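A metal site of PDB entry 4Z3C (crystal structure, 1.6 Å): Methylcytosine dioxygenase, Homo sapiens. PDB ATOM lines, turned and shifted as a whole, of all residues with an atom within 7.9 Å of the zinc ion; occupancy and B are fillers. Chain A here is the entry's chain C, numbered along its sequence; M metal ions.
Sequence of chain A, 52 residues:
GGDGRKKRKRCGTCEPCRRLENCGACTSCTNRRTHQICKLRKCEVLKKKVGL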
ATOM      1  N   LYS A   9     -27.520 -19.619  -0.441  1.00  0.00           N
ATOM      2  CA  LYS A   9     -26.249 -19.860  -1.054  1.00  0.00           C
ATOM      3  C   LYS A   9     -25.239 -20.314  -0.031  1.00  0.00           C
ATOM      4  O   LYS A   9     -25.265 -19.897   1.116  1.00  0.00           O
ATOM      5  CB  LYS A   9     -25.662 -18.518  -1.660  1.00  0.00           C
ATOM      6  CG  LYS A   9     -26.583 -17.667  -2.422  1.00  0.00           C
ATOM      7  CD  LYS A   9     -25.870 -16.364  -2.873  1.00  0.00           C
ATOM      8  N   ARG A  10     -24.335 -21.221  -0.431  1.00  0.00           N
ATOM      9  CA  ARG A  10     -23.227 -21.615   0.435  1.00  0.00           C
ATOM     10  C   ARG A  10     -22.360 -20.419   0.854  1.00  0.00           C
ATOM     11  O   ARG A  10     -22.229 -19.461   0.089  1.00  0.00           O
ATOM     12  CB  ARG A  10     -22.420 -22.698  -0.201  1.00  0.00           C
ATOM     13  CG  ARG A  10     -21.557 -22.277  -1.324  1.00  0.00           C
ATOM     14  CD  ARG A  10     -20.899 -23.505  -1.999  1.00  0.00           C
ATOM     15  NE  ARG A  10     -20.024 -22.934  -3.000  1.00  0.00           N
ATOM     16  CZ  ARG A  10     -18.690 -22.884  -2.951  1.00  0.00           C
ATOM     17  NH1 ARG A  10     -18.040 -22.238  -3.957  1.00  0.00           N
ATOM     18  NH2 ARG A  10     -17.973 -23.477  -1.983  1.00  0.00           N
ATOM     19  N   CYS A  11     -21.761 -20.472   2.016  1.00  0.00           N
ATOM     20  CA  CYS A  11     -20.945 -19.362   2.557  1.00  0.00           C
ATOM     21  C   CYS A  11     -19.598 -19.242   1.808  1.00  0.00           C
ATOM     22  O   CYS A  11     -19.016 -18.151   1.712  1.00  0.00           O
ATOM     23  CB  CYS A  11     -20.733 -19.522   4.057  1.00  0.00           C
ATOM     24  SG  CYS A  11     -19.423 -20.683   4.499  1.00  0.00           S
ATOM     25  N   GLY A  12     -19.081 -20.354   1.269  1.00  0.00           N
ATOM     26  CA  GLY A  12     -17.880 -20.323   0.465  1.00  0.00           C
ATOM     27  C   GLY A  12     -16.573 -20.444   1.247  1.00  0.00           C
ATOM     28  O   GLY A  12     -15.510 -20.654   0.646  1.00  0.00           O
ATOM     29  N   THR A  13     -16.631 -20.297   2.604  1.00  0.00           N
ATOM     30  CA  THR A  13     -15.403 -20.194   3.398  1.00  0.00           C
ATOM     31  C   THR A  13     -15.241 -21.095   4.578  1.00  0.00           C
ATOM     32  O   THR A  13     -14.173 -21.136   5.187  1.00  0.00           O
ATOM     33  CB  THR A  13     -15.222 -18.719   3.879  1.00  0.00           C
ATOM     34  OG1 THR A  13     -16.241 -18.372   4.808  1.00  0.00           O
ATOM     35  CG2 THR A  13     -15.275 -17.802   2.688  1.00  0.00           C
ATOM     36  N   CYS A  14     -16.293 -21.828   4.923  1.00  0.00           N
ATOM     37  CA  CYS A  14     -16.186 -22.834   5.945  1.00  0.00           C
ATOM     38  C   CYS A  14     -15.380 -24.013   5.413  1.00  0.00           C
ATOM     39  O   CYS A  14     -15.151 -24.118   4.194  1.00  0.00           O
ATOM     40  CB  CYS A  14     -17.573 -23.266   6.408  1.00  0.00           C
ATOM     41  SG  CYS A  14     -18.500 -24.230   5.254  1.00  0.00           S
ATOM     42  N   GLU A  15     -14.929 -24.898   6.327  1.00  0.00           N
ATOM     43  CA  GLU A  15     -14.085 -25.970   5.937  1.00  0.00           C
ATOM     44  C   GLU A  15     -14.697 -26.830   4.869  1.00  0.00           C
ATOM     45  O   GLU A  15     -14.031 -27.144   3.912  1.00  0.00           O
ATOM     46  CB  GLU A  15     -13.622 -26.842   7.166  1.00  0.00           C
ATOM     47  CG  GLU A  15     -12.719 -28.038   6.807  1.00  0.00           C
ATOM     48  CD  GLU A  15     -13.432 -29.349   6.390  1.00  0.00           C
ATOM     49  OE1 GLU A  15     -12.765 -30.179   5.697  1.00  0.00           O
ATOM     50  OE2 GLU A  15     -14.633 -29.587   6.698  1.00  0.00           O
ATOM     51  N   PRO A  16     -15.958 -27.263   5.047  1.00  0.00           N
ATOM     52  CA  PRO A  16     -16.593 -28.009   3.969  1.00  0.00           C
ATOM     53  C   PRO A  16     -16.645 -27.239   2.650  1.00  0.00           C
ATOM     54  O   PRO A  16     -16.361 -27.842   1.609  1.00  0.00           O
ATOM     55  CB  PRO A  16     -18.001 -28.248   4.522  1.00  0.00           C
ATOM     56  CG  PRO A  16     -17.821 -28.335   5.955  1.00  0.00           C
ATOM     57  CD  PRO A  16     -16.784 -27.291   6.281  1.00  0.00           C
ATOM     58  N   CYS A  17     -17.004 -25.948   2.681  1.00  0.00           N
ATOM     59  CA  CYS A  17     -17.014 -25.175   1.421  1.00  0.00           C
ATOM     60  C   CYS A  17     -15.707 -25.098   0.701  1.00  0.00           C
ATOM     61  O   CYS A  17     -15.699 -24.850  -0.511  1.00  0.00           O
ATOM     62  CB  CYS A  17     -17.519 -23.729   1.683  1.00  0.00           C
ATOM     63  SG  CYS A  17     -19.323 -23.607   1.789  1.00  0.00           S
ATOM     64  N   ARG A  18     -14.622 -25.081   1.430  1.00  0.00           N
ATOM     65  CA  ARG A  18     -13.275 -25.028   0.838  1.00  0.00           C
ATOM     66  C   ARG A  18     -12.866 -26.284   0.144  1.00  0.00           C
ATOM     67  O   ARG A  18     -11.967 -26.248  -0.678  1.00  0.00           O
ATOM     68  CB  ARG A  18     -12.222 -24.647   1.898  1.00  0.00           C
ATOM     69  CG  ARG A  18     -12.392 -23.267   2.503  1.00  0.00           C
ATOM     70  CD  ARG A  18     -11.396 -23.024   3.592  1.00  0.00           C
ATOM     71  NE  ARG A  18     -11.575 -21.774   4.268  1.00  0.00           N
ATOM     72  CZ  ARG A  18     -10.656 -21.127   4.992  1.00  0.00           C
ATOM     73  NH1 ARG A  18      -9.454 -21.641   5.211  1.00  0.00           N
ATOM     74  NH2 ARG A  18     -10.946 -19.961   5.517  1.00  0.00           N
ATOM     75  N   ARG A  41     -18.725 -31.850   2.133  1.00  0.00           N
ATOM     76  CA  ARG A  41     -18.689 -30.559   1.438  1.00  0.00           C
ATOM     77  C   ARG A  41     -19.881 -29.662   1.809  1.00  0.00           C
ATOM     78  O   ARG A  41     -19.837 -28.474   1.571  1.00  0.00           O
ATOM     79  CB  ARG A  41     -18.669 -30.766  -0.038  1.00  0.00           C
ATOM     80  CG  ARG A  41     -17.483 -31.523  -0.527  1.00  0.00           C
ATOM     81  CD  ARG A  41     -17.502 -31.602  -2.002  1.00  0.00           C
ATOM     82  NE  ARG A  41     -17.073 -30.353  -2.602  1.00  0.00           N
ATOM     83  CZ  ARG A  41     -16.902 -30.158  -3.902  1.00  0.00           C
ATOM     84  NH1 ARG A  41     -16.472 -28.971  -4.322  1.00  0.00           N
ATOM     85  NH2 ARG A  41     -17.111 -31.136  -4.805  1.00  0.00           N
ATOM     86  N   LYS A  42     -20.915 -30.225   2.460  1.00  0.00           N
ATOM     87  CA  LYS A  42     -22.083 -29.444   2.896  1.00  0.00           C
ATOM     88  C   LYS A  42     -21.716 -28.264   3.779  1.00  0.00           C
ATOM     89  O   LYS A  42     -21.017 -28.409   4.766  1.00  0.00           O
ATOM     90  CB  LYS A  42     -23.072 -30.354   3.642  1.00  0.00           C
ATOM     91  CG  LYS A  42     -24.370 -29.727   4.045  1.00  0.00           C
ATOM     92  CD  LYS A  42     -25.271 -29.483   2.871  1.00  0.00           C
ATOM     93  CE  LYS A  42     -26.488 -28.639   3.230  1.00  0.00           C
ATOM     94  NZ  LYS A  42     -27.576 -28.759   2.230  1.00  0.00           N
ATOM     95  N   CYS A  43     -22.180 -27.076   3.382  1.00  0.00           N
ATOM     96  CA  CYS A  43     -21.826 -25.822   4.028  1.00  0.00           C
ATOM     97  C   CYS A  43     -22.332 -25.845   5.465  1.00  0.00           C
ATOM     98  O   CYS A  43     -23.502 -26.187   5.701  1.00  0.00           O
ATOM     99  CB  CYS A  43     -22.383 -24.655   3.220  1.00  0.00           C
ATOM    100  SG  CYS A  43     -22.262 -23.069   4.083  1.00  0.00           S
ATOM    101  N   GLU A  44     -21.493 -25.423   6.406  1.00  0.00           N
ATOM    102  CA  GLU A  44     -21.910 -25.449   7.862  1.00  0.00           C
ATOM    103  C   GLU A  44     -23.093 -24.514   8.116  1.00  0.00           C
ATOM    104  O   GLU A  44     -23.959 -24.777   8.996  1.00  0.00           O
ATOM    105  CB  GLU A  44     -20.738 -25.112   8.777  1.00  0.00           C
ATOM    106  CG  GLU A  44     -19.518 -26.052   8.655  1.00  0.00           C
ATOM    107  CD  GLU A  44     -19.688 -27.429   9.290  1.00  0.00           C
ATOM    108  OE1 GLU A  44     -20.824 -27.846   9.649  1.00  0.00           O
ATOM    109  OE2 GLU A  44     -18.644 -28.113   9.440  1.00  0.00           O
ATOM    110  N   VAL A  45     -23.160 -23.427   7.350  1.00  0.00           N
ATOM    111  CA  VAL A  45     -24.234 -22.434   7.505  1.00  0.00           C
ATOM    112  C   VAL A  45     -25.565 -23.033   7.053  1.00  0.00           C
ATOM    113  O   VAL A  45     -26.623 -22.854   7.702  1.00  0.00           O
ATOM    114  CB  VAL A  45     -23.892 -21.162   6.705  1.00  0.00           C
ATOM    115  CG1 VAL A  45     -24.985 -20.124   6.876  1.00  0.00           C
ATOM    116  CG2 VAL A  45     -22.528 -20.601   7.157  1.00  0.00           C
ATOM    117  N   LEU A  46     -25.542 -23.743   5.923  1.00  0.00           N
ATOM    118  CA  LEU A  46     -26.725 -24.341   5.327  1.00  0.00           C
ATOM    119  C   LEU A  46     -27.265 -25.527   6.135  1.00  0.00           C
ATOM    120  O   LEU A  46     -28.394 -25.972   5.897  1.00  0.00           O
ATOM    121  CB  LEU A  46     -26.475 -24.769   3.862  1.00  0.00           C
ATOM    122  CG  LEU A  46     -26.097 -23.661   2.898  1.00  0.00           C
ATOM    123  CD1 LEU A  46     -25.936 -24.185   1.484  1.00  0.00           C
ATOM    124  CD2 LEU A  46     -27.129 -22.558   2.955  1.00  0.00           C
HETATM  125 ZN    ZN M   1     -19.848 -22.812   3.981  1.00  0.00          ZN
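NH2 of Arg 10 lies within hydrogen-bond range of O of Cys 17 (3.0 Å). SG of Cys 17 lies close to N of Gly 12, at 3.3 Å. The backbone NH (N) of Glu 44 lies close to the side-chain sulfur (SG) of Cys 14 (3.4 Å). The backbone NH (N) of Thr 13 lies close to the side-chain sulfur (SG) of Cys 11 (3.4 Å). The backbone NH (N) of Val 45 sits close to the side-chain sulfur (SG) of Cys 43 (3.4 Å).
Merely in contact with the zinc ion: Gly 12 (3.7 Å) and Glu 44 (3.9 Å). The nearest printed residue that does not touch the zinc ion is Thr 13 (4.3 Å).
SG of Cys 11 is bound to the zinc ion (2.2 Å). The side-chain sulfur (SG) of Cys 14 is bound to the zinc ion (2.3 Å). The zinc ion is bound by the side-chain sulfur (SG) of Cys 17, at 2.4 Å. The zinc ion is bound by the side-chain sulfur (SG) of Cys 43 (2.4 Å).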
